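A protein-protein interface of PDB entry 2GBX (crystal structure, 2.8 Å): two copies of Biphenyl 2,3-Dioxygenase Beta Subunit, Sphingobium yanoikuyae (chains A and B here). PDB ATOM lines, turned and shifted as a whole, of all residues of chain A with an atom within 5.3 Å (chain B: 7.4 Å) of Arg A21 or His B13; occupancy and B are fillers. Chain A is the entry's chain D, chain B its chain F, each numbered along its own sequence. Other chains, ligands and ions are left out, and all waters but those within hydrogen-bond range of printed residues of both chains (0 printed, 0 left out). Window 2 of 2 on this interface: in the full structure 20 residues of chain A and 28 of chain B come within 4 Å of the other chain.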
ATOM      1  N   TYR A  14      13.378 -29.498 -19.715  1.00  0.00           N
ATOM      2  CA  TYR A  14      12.264 -28.583 -19.455  1.00  0.00           C
ATOM      3  C   TYR A  14      11.176 -29.241 -18.603  1.00  0.00           C
ATOM      4  O   TYR A  14      10.635 -28.615 -17.690  1.00  0.00           O
ATOM      5  CB  TYR A  14      11.659 -28.081 -20.771  1.00  0.00           C
ATOM      6  CG  TYR A  14      10.460 -27.174 -20.588  1.00  0.00           C
ATOM      7  CD1 TYR A  14      10.615 -25.792 -20.493  1.00  0.00           C
ATOM      8  CD2 TYR A  14       9.172 -27.699 -20.505  1.00  0.00           C
ATOM      9  CE1 TYR A  14       9.516 -24.957 -20.322  1.00  0.00           C
ATOM     10  CE2 TYR A  14       8.069 -26.876 -20.332  1.00  0.00           C
ATOM     11  CZ  TYR A  14       8.247 -25.507 -20.242  1.00  0.00           C
ATOM     12  OH  TYR A  14       7.152 -24.691 -20.074  1.00  0.00           O
ATOM     13  N   ILE A  16      11.511 -31.687 -16.494  1.00  0.00           N
ATOM     14  CA  ILE A  16      12.039 -31.858 -15.137  1.00  0.00           C
ATOM     15  C   ILE A  16      12.034 -30.528 -14.378  1.00  0.00           C
ATOM     16  O   ILE A  16      11.745 -30.495 -13.180  1.00  0.00           O
ATOM     17  CB  ILE A  16      13.469 -32.448 -15.156  1.00  0.00           C
ATOM     18  CG1 ILE A  16      13.444 -33.873 -15.712  1.00  0.00           C
ATOM     19  CG2 ILE A  16      14.072 -32.455 -13.756  1.00  0.00           C
ATOM     20  CD1 ILE A  16      14.813 -34.497 -15.862  1.00  0.00           C
ATOM     21  N   GLU A  17      12.360 -29.441 -15.077  1.00  0.00           N
ATOM     22  CA  GLU A  17      12.272 -28.095 -14.504  1.00  0.00           C
ATOM     23  C   GLU A  17      10.826 -27.751 -14.150  1.00  0.00           C
ATOM     24  O   GLU A  17      10.548 -27.268 -13.053  1.00  0.00           O
ATOM     25  CB  GLU A  17      12.828 -27.050 -15.478  1.00  0.00           C
ATOM     26  CG  GLU A  17      14.348 -27.058 -15.615  1.00  0.00           C
ATOM     27  CD  GLU A  17      15.048 -26.206 -14.566  1.00  0.00           C
ATOM     28  OE1 GLU A  17      14.558 -26.133 -13.418  1.00  0.00           O
ATOM     29  OE2 GLU A  17      16.096 -25.611 -14.892  1.00  0.00           O
ATOM     30  N   ALA A  18       9.915 -28.014 -15.085  1.00  0.00           N
ATOM     31  CA  ALA A  18       8.483 -27.785 -14.872  1.00  0.00           C
ATOM     32  C   ALA A  18       7.918 -28.673 -13.762  1.00  0.00           C
ATOM     33  O   ALA A  18       6.993 -28.271 -13.054  1.00  0.00           O
ATOM     34  CB  ALA A  18       7.713 -28.008 -16.168  1.00  0.00           C
ATOM     35  N   HIS A  19       8.473 -29.875 -13.621  1.00  0.00           N
ATOM     36  CA  HIS A  19       8.086 -30.790 -12.547  1.00  0.00           C
ATOM     37  C   HIS A  19       8.492 -30.240 -11.179  1.00  0.00           C
ATOM     38  O   HIS A  19       7.705 -30.289 -10.233  1.00  0.00           O
ATOM     39  CB  HIS A  19       8.703 -32.175 -12.772  1.00  0.00           C
ATOM     40  CG  HIS A  19       8.469 -33.133 -11.644  1.00  0.00           C
ATOM     41  ND1 HIS A  19       7.276 -33.804 -11.471  1.00  0.00           N
ATOM     42  CD2 HIS A  19       9.277 -33.535 -10.634  1.00  0.00           C
ATOM     43  CE1 HIS A  19       7.359 -34.575 -10.402  1.00  0.00           C
ATOM     44  NE2 HIS A  19       8.563 -34.431  -9.876  1.00  0.00           N
ATOM     45  N   TYR A  20       9.715 -29.720 -11.081  1.00  0.00           N
ATOM     46  CA  TYR A  20      10.204 -29.125  -9.833  1.00  0.00           C
ATOM     47  C   TYR A  20       9.507 -27.803  -9.508  1.00  0.00           C
ATOM     48  O   TYR A  20       9.278 -27.497  -8.335  1.00  0.00           O
ATOM     49  CB  TYR A  20      11.724 -28.906  -9.878  1.00  0.00           C
ATOM     50  CG  TYR A  20      12.557 -30.175  -9.829  1.00  0.00           C
ATOM     51  CD1 TYR A  20      12.289 -31.178  -8.892  1.00  0.00           C
ATOM     52  CD2 TYR A  20      13.635 -30.360 -10.701  1.00  0.00           C
ATOM     53  CE1 TYR A  20      13.057 -32.335  -8.840  1.00  0.00           C
ATOM     54  CE2 TYR A  20      14.410 -31.514 -10.656  1.00  0.00           C
ATOM     55  CZ  TYR A  20      14.117 -32.497  -9.724  1.00  0.00           C
ATOM     56  OH  TYR A  20      14.880 -33.641  -9.673  1.00  0.00           O
ATOM     57  N   ARG A  21       9.183 -27.020 -10.537  1.00  0.00           N
ATOM     58  CA  ARG A  21       8.440 -25.768 -10.350  1.00  0.00           C
ATOM     59  C   ARG A  21       7.058 -26.033  -9.755  1.00  0.00           C
ATOM     60  O   ARG A  21       6.620 -25.321  -8.848  1.00  0.00           O
ATOM     61  CB  ARG A  21       8.293 -25.003 -11.672  1.00  0.00           C
ATOM     62  CG  ARG A  21       9.534 -24.233 -12.099  1.00  0.00           C
ATOM     63  CD  ARG A  21       9.192 -23.143 -13.107  1.00  0.00           C
ATOM     64  NE  ARG A  21       8.526 -23.671 -14.298  1.00  0.00           N
ATOM     65  CZ  ARG A  21       9.141 -24.249 -15.331  1.00  0.00           C
ATOM     66  NH1 ARG A  21      10.464 -24.400 -15.348  1.00  0.00           N
ATOM     67  NH2 ARG A  21       8.423 -24.688 -16.360  1.00  0.00           N
ATOM     68  N   ALA A  22       6.378 -27.052 -10.275  1.00  0.00           N
ATOM     69  CA  ALA A  22       5.089 -27.481  -9.735  1.00  0.00           C
ATOM     70  C   ALA A  22       5.254 -28.030  -8.321  1.00  0.00           C
ATOM     71  O   ALA A  22       4.454 -27.730  -7.439  1.00  0.00           O
ATOM     72  CB  ALA A  22       4.457 -28.530 -10.639  1.00  0.00           C
ATOM     73  N   GLU A  23       6.305 -28.822  -8.114  1.00  0.00           N
ATOM     74  CA  GLU A  23       6.599 -29.418  -6.808  1.00  0.00           C
ATOM     75  C   GLU A  23       6.824 -28.356  -5.732  1.00  0.00           C
ATOM     76  O   GLU A  23       6.359 -28.504  -4.600  1.00  0.00           O
ATOM     77  CB  GLU A  23       7.831 -30.321  -6.909  1.00  0.00           C
ATOM     78  CG  GLU A  23       8.020 -31.254  -5.733  1.00  0.00           C
ATOM     79  CD  GLU A  23       9.228 -32.150  -5.901  1.00  0.00           C
ATOM     80  OE1 GLU A  23      10.363 -31.630  -5.859  1.00  0.00           O
ATOM     81  OE2 GLU A  23       9.040 -33.373  -6.076  1.00  0.00           O
ATOM     82  N   VAL A  24       7.542 -27.295  -6.092  1.00  0.00           N
ATOM     83  CA  VAL A  24       7.785 -26.173  -5.186  1.00  0.00           C
ATOM     84  C   VAL A  24       6.487 -25.444  -4.832  1.00  0.00           C
ATOM     85  O   VAL A  24       6.283 -25.061  -3.679  1.00  0.00           O
ATOM     86  CB  VAL A  24       8.797 -25.173  -5.793  1.00  0.00           C
ATOM     87  CG1 VAL A  24       8.783 -23.852  -5.033  1.00  0.00           C
ATOM     88  CG2 VAL A  24      10.194 -25.775  -5.802  1.00  0.00           C
ATOM     89  N   ARG A  25       5.613 -25.262  -5.821  1.00  0.00           N
ATOM     90  CA  ARG A  25       4.316 -24.611  -5.605  1.00  0.00           C
ATOM     91  C   ARG A  25       3.443 -25.380  -4.609  1.00  0.00           C
ATOM     92  O   ARG A  25       2.710 -24.771  -3.827  1.00  0.00           O
ATOM     93  CB  ARG A  25       3.573 -24.429  -6.936  1.00  0.00           C
ATOM     94  CG  ARG A  25       2.178 -23.822  -6.801  1.00  0.00           C
ATOM     95  CD  ARG A  25       1.675 -23.240  -8.118  1.00  0.00           C
ATOM     96  NE  ARG A  25       1.667 -24.221  -9.204  1.00  0.00           N
ATOM     97  CZ  ARG A  25       0.752 -25.179  -9.366  1.00  0.00           C
ATOM     98  NH1 ARG A  25      -0.260 -25.317  -8.512  1.00  0.00           N
ATOM     99  NH2 ARG A  25       0.853 -26.011 -10.397  1.00  0.00           N
ATOM    100  N   VAL B   8       1.059 -23.198 -20.187  1.00  0.00           N
ATOM    101  CA  VAL B   8       1.534 -22.733 -21.493  1.00  0.00           C
ATOM    102  C   VAL B   8       2.582 -23.678 -22.081  1.00  0.00           C
ATOM    103  O   VAL B   8       3.216 -24.446 -21.354  1.00  0.00           O
ATOM    104  CB  VAL B   8       2.130 -21.305 -21.416  1.00  0.00           C
ATOM    105  CG1 VAL B   8       1.077 -20.313 -20.947  1.00  0.00           C
ATOM    106  CG2 VAL B   8       3.353 -21.275 -20.503  1.00  0.00           C
ATOM    107  N   THR B   9       2.755 -23.609 -23.399  1.00  0.00           N
ATOM    108  CA  THR B   9       3.715 -24.459 -24.105  1.00  0.00           C
ATOM    109  C   THR B   9       5.154 -24.011 -23.826  1.00  0.00           C
ATOM    110  O   THR B   9       5.377 -22.858 -23.449  1.00  0.00           O
ATOM    111  CB  THR B   9       3.463 -24.440 -25.628  1.00  0.00           C
ATOM    112  OG1 THR B   9       3.484 -23.089 -26.106  1.00  0.00           O
ATOM    113  CG2 THR B   9       2.117 -25.070 -25.956  1.00  0.00           C
ATOM    114  N   PRO B  10       6.136 -24.920 -24.005  1.00  0.00           N
ATOM    115  CA  PRO B  10       7.550 -24.586 -23.783  1.00  0.00           C
ATOM    116  C   PRO B  10       8.048 -23.362 -24.560  1.00  0.00           C
ATOM    117  O   PRO B  10       8.891 -22.618 -24.055  1.00  0.00           O
ATOM    118  CB  PRO B  10       8.286 -25.846 -24.253  1.00  0.00           C
ATOM    119  CG  PRO B  10       7.304 -26.937 -24.100  1.00  0.00           C
ATOM    120  CD  PRO B  10       5.971 -26.331 -24.406  1.00  0.00           C
ATOM    121  N   ASP B  11       7.535 -23.166 -25.774  1.00  0.00           N
ATOM    122  CA  ASP B  11       7.908 -22.014 -26.600  1.00  0.00           C
ATOM    123  C   ASP B  11       7.402 -20.704 -25.996  1.00  0.00           C
ATOM    124  O   ASP B  11       8.108 -19.694 -26.012  1.00  0.00           O
ATOM    125  CB  ASP B  11       7.366 -22.171 -28.026  1.00  0.00           C
ATOM    126  CG  ASP B  11       7.975 -23.355 -28.762  1.00  0.00           C
ATOM    127  OD1 ASP B  11       9.176 -23.641 -28.560  1.00  0.00           O
ATOM    128  OD2 ASP B  11       7.251 -23.996 -29.552  1.00  0.00           O
ATOM    129  N   VAL B  12       6.181 -20.729 -25.466  1.00  0.00           N
ATOM    130  CA  VAL B  12       5.588 -19.561 -24.811  1.00  0.00           C
ATOM    131  C   VAL B  12       6.241 -19.299 -23.451  1.00  0.00           C
ATOM    132  O   VAL B  12       6.399 -18.146 -23.047  1.00  0.00           O
ATOM    133  CB  VAL B  12       4.061 -19.732 -24.625  1.00  0.00           C
ATOM    134  CG1 VAL B  12       3.466 -18.538 -23.888  1.00  0.00           C
ATOM    135  CG2 VAL B  12       3.378 -19.915 -25.973  1.00  0.00           C
ATOM    136  N   HIS B  13       6.619 -20.372 -22.755  1.00  0.00           N
ATOM    137  CA  HIS B  13       7.270 -20.269 -21.445  1.00  0.00           C
ATOM    138  C   HIS B  13       8.599 -19.516 -21.518  1.00  0.00           C
ATOM    139  O   HIS B  13       8.928 -18.746 -20.613  1.00  0.00           O
ATOM    140  CB  HIS B  13       7.496 -21.663 -20.851  1.00  0.00           C
ATOM    141  CG  HIS B  13       8.009 -21.648 -19.445  1.00  0.00           C
ATOM    142  ND1 HIS B  13       9.351 -21.554 -19.142  1.00  0.00           N
ATOM    143  CD2 HIS B  13       7.361 -21.724 -18.258  1.00  0.00           C
ATOM    144  CE1 HIS B  13       9.506 -21.567 -17.830  1.00  0.00           C
ATOM    145  NE2 HIS B  13       8.315 -21.671 -17.271  1.00  0.00           N
ATOM    146  N   TYR B  14       9.358 -19.745 -22.588  1.00  0.00           N
ATOM    147  CA  TYR B  14      10.626 -19.047 -22.800  1.00  0.00           C
ATOM    148  C   TYR B  14      10.411 -17.553 -23.044  1.00  0.00           C
ATOM    149  O   TYR B  14      11.173 -16.723 -22.546  1.00  0.00           O
ATOM    150  CB  TYR B  14      11.395 -19.653 -23.979  1.00  0.00           C
ATOM    151  CG  TYR B  14      12.704 -18.948 -24.271  1.00  0.00           C
ATOM    152  CD1 TYR B  14      13.879 -19.325 -23.629  1.00  0.00           C
ATOM    153  CD2 TYR B  14      12.762 -17.893 -25.180  1.00  0.00           C
ATOM    154  CE1 TYR B  14      15.079 -18.677 -23.889  1.00  0.00           C
ATOM    155  CE2 TYR B  14      13.957 -17.236 -25.445  1.00  0.00           C
ATOM    156  CZ  TYR B  14      15.111 -17.632 -24.795  1.00  0.00           C
ATOM    157  OH  TYR B  14      16.300 -16.989 -25.057  1.00  0.00           O
ATOM    158  N   ASP B  15       9.381 -17.220 -23.819  1.00  0.00           N
ATOM    159  CA  ASP B  15       9.069 -15.826 -24.141  1.00  0.00           C
ATOM    160  C   ASP B  15       8.687 -15.031 -22.891  1.00  0.00           C
ATOM    161  O   ASP B  15       9.036 -13.855 -22.767  1.00  0.00           O
ATOM    162  CB  ASP B  15       7.944 -15.749 -25.182  1.00  0.00           C
ATOM    163  CG  ASP B  15       8.332 -16.365 -26.518  1.00  0.00           C
ATOM    164  OD1 ASP B  15       9.393 -17.021 -26.597  1.00  0.00           O
ATOM    165  OD2 ASP B  15       7.569 -16.195 -27.492  1.00  0.00           O
ATOM    166  N   ILE B  16       7.971 -15.677 -21.971  1.00  0.00           N
ATOM    167  CA  ILE B  16       7.622 -15.070 -20.684  1.00  0.00           C
ATOM    168  C   ILE B  16       8.848 -15.008 -19.768  1.00  0.00           C
ATOM    169  O   ILE B  16       9.034 -14.029 -19.040  1.00  0.00           O
ATOM    170  CB  ILE B  16       6.486 -15.847 -19.978  1.00  0.00           C
ATOM    171  CG1 ILE B  16       5.196 -15.770 -20.800  1.00  0.00           C
ATOM    172  CG2 ILE B  16       6.237 -15.290 -18.581  1.00  0.00           C
ATOM    173  CD1 ILE B  16       4.051 -16.572 -20.217  1.00  0.00           C
ATOM    174  N   GLU B  17       9.672 -16.054 -19.803  1.00  0.00           N
ATOM    175  CA  GLU B  17      10.931 -16.078 -19.051  1.00  0.00           C
ATOM    176  C   GLU B  17      11.883 -14.983 -19.527  1.00  0.00           C
ATOM    177  O   GLU B  17      12.462 -14.260 -18.716  1.00  0.00           O
ATOM    178  CB  GLU B  17      11.613 -17.447 -19.173  1.00  0.00           C
ATOM    179  CG  GLU B  17      11.056 -18.517 -18.238  1.00  0.00           C
ATOM    180  CD  GLU B  17      11.650 -18.459 -16.836  1.00  0.00           C
ATOM    181  OE1 GLU B  17      12.102 -17.372 -16.407  1.00  0.00           O
ATOM    182  OE2 GLU B  17      11.664 -19.510 -16.158  1.00  0.00           O
ATOM    183  N   ALA B  18      12.035 -14.866 -20.845  1.00  0.00           N
ATOM    184  CA  ALA B  18      12.888 -13.840 -21.449  1.00  0.00           C
ATOM    185  C   ALA B  18      12.348 -12.429 -21.206  1.00  0.00           C
ATOM    186  O   ALA B  18      13.121 -11.472 -21.129  1.00  0.00           O
ATOM    187  CB  ALA B  18      13.042 -14.093 -22.943  1.00  0.00           C
ATOM    188  N   HIS B  19      11.027 -12.306 -21.092  1.00  0.00           N
ATOM    189  CA  HIS B  19      10.387 -11.023 -20.800  1.00  0.00           C
ATOM    190  C   HIS B  19      10.710 -10.551 -19.383  1.00  0.00           C
ATOM    191  O   HIS B  19      11.060  -9.386 -19.181  1.00  0.00           O
ATOM    192  CB  HIS B  19       8.868 -11.119 -20.992  1.00  0.00           C
ATOM    193  CG  HIS B  19       8.131  -9.871 -20.615  1.00  0.00           C
ATOM    194  ND1 HIS B  19       8.051  -8.774 -21.447  1.00  0.00           N
ATOM    195  CD2 HIS B  19       7.442  -9.546 -19.496  1.00  0.00           C
ATOM    196  CE1 HIS B  19       7.343  -7.828 -20.856  1.00  0.00           C
ATOM    197  NE2 HIS B  19       6.962  -8.270 -19.671  1.00  0.00           N
ATOM    198  N   TYR B  20      10.588 -11.453 -18.409  1.00  0.00           N
ATOM    199  CA  TYR B  20      10.922 -11.135 -17.017  1.00  0.00           C
ATOM    200  C   TYR B  20      12.415 -10.864 -16.835  1.00  0.00           C
ATOM    201  O   TYR B  20      12.798 -10.048 -15.996  1.00  0.00           O
ATOM    202  CB  TYR B  20      10.483 -12.258 -16.067  1.00  0.00           C
ATOM    203  CG  TYR B  20       8.985 -12.367 -15.849  1.00  0.00           C
ATOM    204  CD1 TYR B  20       8.218 -11.240 -15.539  1.00  0.00           C
ATOM    205  CD2 TYR B  20       8.338 -13.605 -15.924  1.00  0.00           C
ATOM    206  CE1 TYR B  20       6.847 -11.342 -15.332  1.00  0.00           C
ATOM    207  CE2 TYR B  20       6.969 -13.716 -15.716  1.00  0.00           C
ATOM    208  CZ  TYR B  20       6.229 -12.581 -15.421  1.00  0.00           C
ATOM    209  OH  TYR B  20       4.872 -12.687 -15.214  1.00  0.00           O
ATOM    210  N   ARG B  21      13.251 -11.553 -17.610  1.00  0.00           N
ATOM    211  CA  ARG B  21      14.696 -11.320 -17.576  1.00  0.00           C
ATOM    212  C   ARG B  21      15.052  -9.935 -18.117  1.00  0.00           C
ATOM    213  O   ARG B  21      15.905  -9.245 -17.553  1.00  0.00           O
ATOM    214  CB  ARG B  21      15.454 -12.402 -18.357  1.00  0.00           C
ATOM    215  CG  ARG B  21      15.609 -13.718 -17.604  1.00  0.00           C
ATOM    216  CD  ARG B  21      16.702 -14.583 -18.217  1.00  0.00           C
ATOM    217  NE  ARG B  21      16.360 -15.030 -19.569  1.00  0.00           N
ATOM    218  CZ  ARG B  21      15.693 -16.147 -19.867  1.00  0.00           C
ATOM    219  NH1 ARG B  21      15.269 -16.975 -18.914  1.00  0.00           N
ATOM    220  NH2 ARG B  21      15.445 -16.442 -21.139  1.00  0.00           N
ATOM    221  N   SER B 104      12.341 -16.814  -9.964  1.00  0.00           N
ATOM    222  CA  SER B 104      12.278 -18.276  -9.979  1.00  0.00           C
ATOM    223  C   SER B 104      10.830 -18.764  -9.982  1.00  0.00           C
ATOM    224  O   SER B 104       9.909 -18.000  -9.691  1.00  0.00           O
ATOM    225  CB  SER B 104      13.018 -18.849  -8.767  1.00  0.00           C
ATOM    226  OG  SER B 104      13.060 -20.265  -8.814  1.00  0.00           O
ATOM    227  N   ASN B 105      10.645 -20.043 -10.310  1.00  0.00           N
ATOM    228  CA  ASN B 105       9.320 -20.671 -10.367  1.00  0.00           C
ATOM    229  C   ASN B 105       8.332 -19.939 -11.284  1.00  0.00           C
ATOM    230  O   ASN B 105       7.186 -19.682 -10.905  1.00  0.00           O
ATOM    231  CB  ASN B 105       8.740 -20.843  -8.953  1.00  0.00           C
ATOM    232  CG  ASN B 105       9.038 -22.206  -8.363  1.00  0.00           C
ATOM    233  OD1 ASN B 105      10.193 -22.622  -8.278  1.00  0.00           O
ATOM    234  ND2 ASN B 105       7.990 -22.910  -7.953  1.00  0.00           N
ATOM    235  N   VAL B 106       8.782 -19.618 -12.493  1.00  0.00           N
ATOM    236  CA  VAL B 106       7.940 -18.933 -13.472  1.00  0.00           C
ATOM    237  C   VAL B 106       6.979 -19.933 -14.121  1.00  0.00           C
ATOM    238  O   VAL B 106       7.305 -20.556 -15.131  1.00  0.00           O
ATOM    239  CB  VAL B 106       8.786 -18.227 -14.560  1.00  0.00           C
ATOM    240  CG1 VAL B 106       7.887 -17.506 -15.556  1.00  0.00           C
ATOM    241  CG2 VAL B 106       9.762 -17.249 -13.922  1.00  0.00           C
ATOM    242  N   GLU B 107       5.798 -20.083 -13.520  1.00  0.00           N
ATOM    243  CA  GLU B 107       4.767 -20.988 -14.031  1.00  0.00           C
ATOM    244  C   GLU B 107       3.597 -20.197 -14.612  1.00  0.00           C
ATOM    245  O   GLU B 107       2.866 -19.527 -13.879  1.00  0.00           O
ATOM    246  CB  GLU B 107       4.276 -21.919 -12.920  1.00  0.00           C
ATOM    247  CG  GLU B 107       5.220 -23.074 -12.634  1.00  0.00           C
ATOM    248  CD  GLU B 107       4.723 -23.974 -11.520  1.00  0.00           C
ATOM    249  OE1 GLU B 107       4.709 -23.522 -10.355  1.00  0.00           O
ATOM    250  OE2 GLU B 107       4.359 -25.135 -11.809  1.00  0.00           O
ATOM    251  N   ALA B 108       3.427 -20.286 -15.931  1.00  0.00           N
ATOM    252  CA  ALA B 108       2.373 -19.561 -16.640  1.00  0.00           C
ATOM    253  C   ALA B 108       1.189 -20.474 -16.954  1.00  0.00           C
ATOM    254  O   ALA B 108       1.364 -21.668 -17.206  1.00  0.00           O
ATOM    255  CB  ALA B 108       2.925 -18.959 -17.923  1.00  0.00           C
ATOM    256  N   LEU B 116      -2.562 -14.395 -19.914  1.00  0.00           N
ATOM    257  CA  LEU B 116      -1.736 -15.406 -19.251  1.00  0.00           C
ATOM    258  C   LEU B 116      -1.574 -15.137 -17.755  1.00  0.00           C
ATOM    259  O   LEU B 116      -0.977 -14.135 -17.361  1.00  0.00           O
ATOM    260  CB  LEU B 116      -0.352 -15.459 -19.905  1.00  0.00           C
ATOM    261  CG  LEU B 116      -0.306 -15.930 -21.361  1.00  0.00           C
ATOM    262  CD1 LEU B 116       1.051 -15.634 -21.979  1.00  0.00           C
ATOM    263  CD2 LEU B 116      -0.628 -17.413 -21.456  1.00  0.00           C
ATOM    264  N   LEU B 119       2.510 -17.140 -12.215  1.00  0.00           N
ATOM    265  CA  LEU B 119       3.015 -17.154 -10.841  1.00  0.00           C
ATOM    266  C   LEU B 119       4.541 -17.120 -10.871  1.00  0.00           C
ATOM    267  O   LEU B 119       5.156 -17.653 -11.797  1.00  0.00           O
ATOM    268  CB  LEU B 119       2.544 -18.416 -10.112  1.00  0.00           C
ATOM    269  CG  LEU B 119       1.038 -18.695 -10.124  1.00  0.00           C
ATOM    270  CD1 LEU B 119       0.741 -20.025  -9.447  1.00  0.00           C
ATOM    271  CD2 LEU B 119       0.271 -17.568  -9.449  1.00  0.00           C
ATOM    272  N   ASN B 121       8.295 -16.613  -8.089  1.00  0.00           N
ATOM    273  CA  ASN B 121       9.010 -16.316  -6.847  1.00  0.00           C
ATOM    274  C   ASN B 121      10.123 -15.310  -7.123  1.00  0.00           C
ATOM    275  O   ASN B 121      10.816 -15.416  -8.137  1.00  0.00           O
ATOM    276  CB  ASN B 121       9.620 -17.594  -6.263  1.00  0.00           C
ATOM    277  CG  ASN B 121       8.583 -18.673  -5.995  1.00  0.00           C
ATOM    278  OD1 ASN B 121       7.397 -18.500  -6.278  1.00  0.00           O
ATOM    279  ND2 ASN B 121       9.032 -19.797  -5.448  1.00  0.00           N
ATOM    280  N   PHE B 151       5.200  -8.706 -24.337  1.00  0.00           N
ATOM    281  CA  PHE B 151       4.171  -8.804 -23.322  1.00  0.00           C
ATOM    282  C   PHE B 151       3.991  -7.484 -22.618  1.00  0.00           C
ATOM    283  O   PHE B 151       4.865  -6.636 -22.662  1.00  0.00           O
ATOM    284  CB  PHE B 151       4.524  -9.884 -22.319  1.00  0.00           C
ATOM    285  CG  PHE B 151       4.569 -11.251 -22.906  1.00  0.00           C
ATOM    286  CD1 PHE B 151       3.408 -11.959 -23.134  1.00  0.00           C
ATOM    287  CD2 PHE B 151       5.771 -11.828 -23.239  1.00  0.00           C
ATOM    288  CE1 PHE B 151       3.447 -13.206 -23.675  1.00  0.00           C
ATOM    289  CE2 PHE B 151       5.812 -13.072 -23.776  1.00  0.00           C
ATOM    290  CZ  PHE B 151       4.649 -13.763 -23.995  1.00  0.00           C
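A ring nitrogen (NE2) of His B13 is in hydrogen-bond range of the guanidinium group (NH2) of Arg A21, 3.2 Å away.
O of Arg A21 is in hydrogen-bond range of ND2 of Asn B105 (2.9 Å).
The backbone carbonyl oxygen (O) of Val B106 lies within hydrogen-bond range of the guanidinium group (NE) of Arg A21 (3.4 Å).
N of Ala A22 is in hydrogen-bond range of OE2 of Glu B107, at 3.2 Å.
The side-chain carboxylate (OE1) of Glu B107 lies within salt-bridge range of the guanidinium group (NE) of Arg A25.
O of Arg A21 lies close to OE1 of Glu B107 (3.0 Å).
The backbone carbonyl oxygen (O) of Val B106 lies within hydrogen-bond range of a ring nitrogen (NE2) of His B13 (2.6 Å).
The backbone NH (N) of Leu B119 lies within hydrogen-bond range of the backbone carbonyl oxygen (O) of Glu B107 (2.9 Å).
Among the printed residues, merely in contact across the chains: Tyr A14 with Pro B10 (3.7 Å), Tyr A14 with His B13 (3.1 Å), Val A24 with Asn B105 (3.2 Å), Arg A25 with Asn B105 (3.97 Å) and Arg A25 with Leu B119 (3.6 Å).
Of the printed residues of chain B, Tyr A14 touches Pro B10 and His B13.
Of chain B, only His B13 (3.2 Å), Asn B105 (2.9 Å), Val B106 (3.4 Å) and Glu B107 (3.0 Å) come within 4 Å of Arg A21.
Of the printed residues of chain B, Ala A22 touches Glu B107 (3.2 Å).
Of the printed residues of chain B, Arg A25 touches Asn B105, Glu B107 and Leu B119.
Of the printed residues of chain A, Pro B10 touches Tyr A14.
His B13 touches just these residues of chain A: Tyr A14 (3.1 Å) and Arg A21 (3.2 Å).
Printed residues of chain A within 4 Å of Glu B107: Arg A21 (3.0 Å), Ala A22 (3.2 Å) and Arg A25 (3.3 Å).
The nearest printed residue of chain B that does not touch Val A24 is Asn B121 (4.1 Å).
Of the 11 printed residues of chain A, 5 touch a printed residue of chain B.
Positions printed for both chains: 14, 16, 17, 18, 19, 20 and 21.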
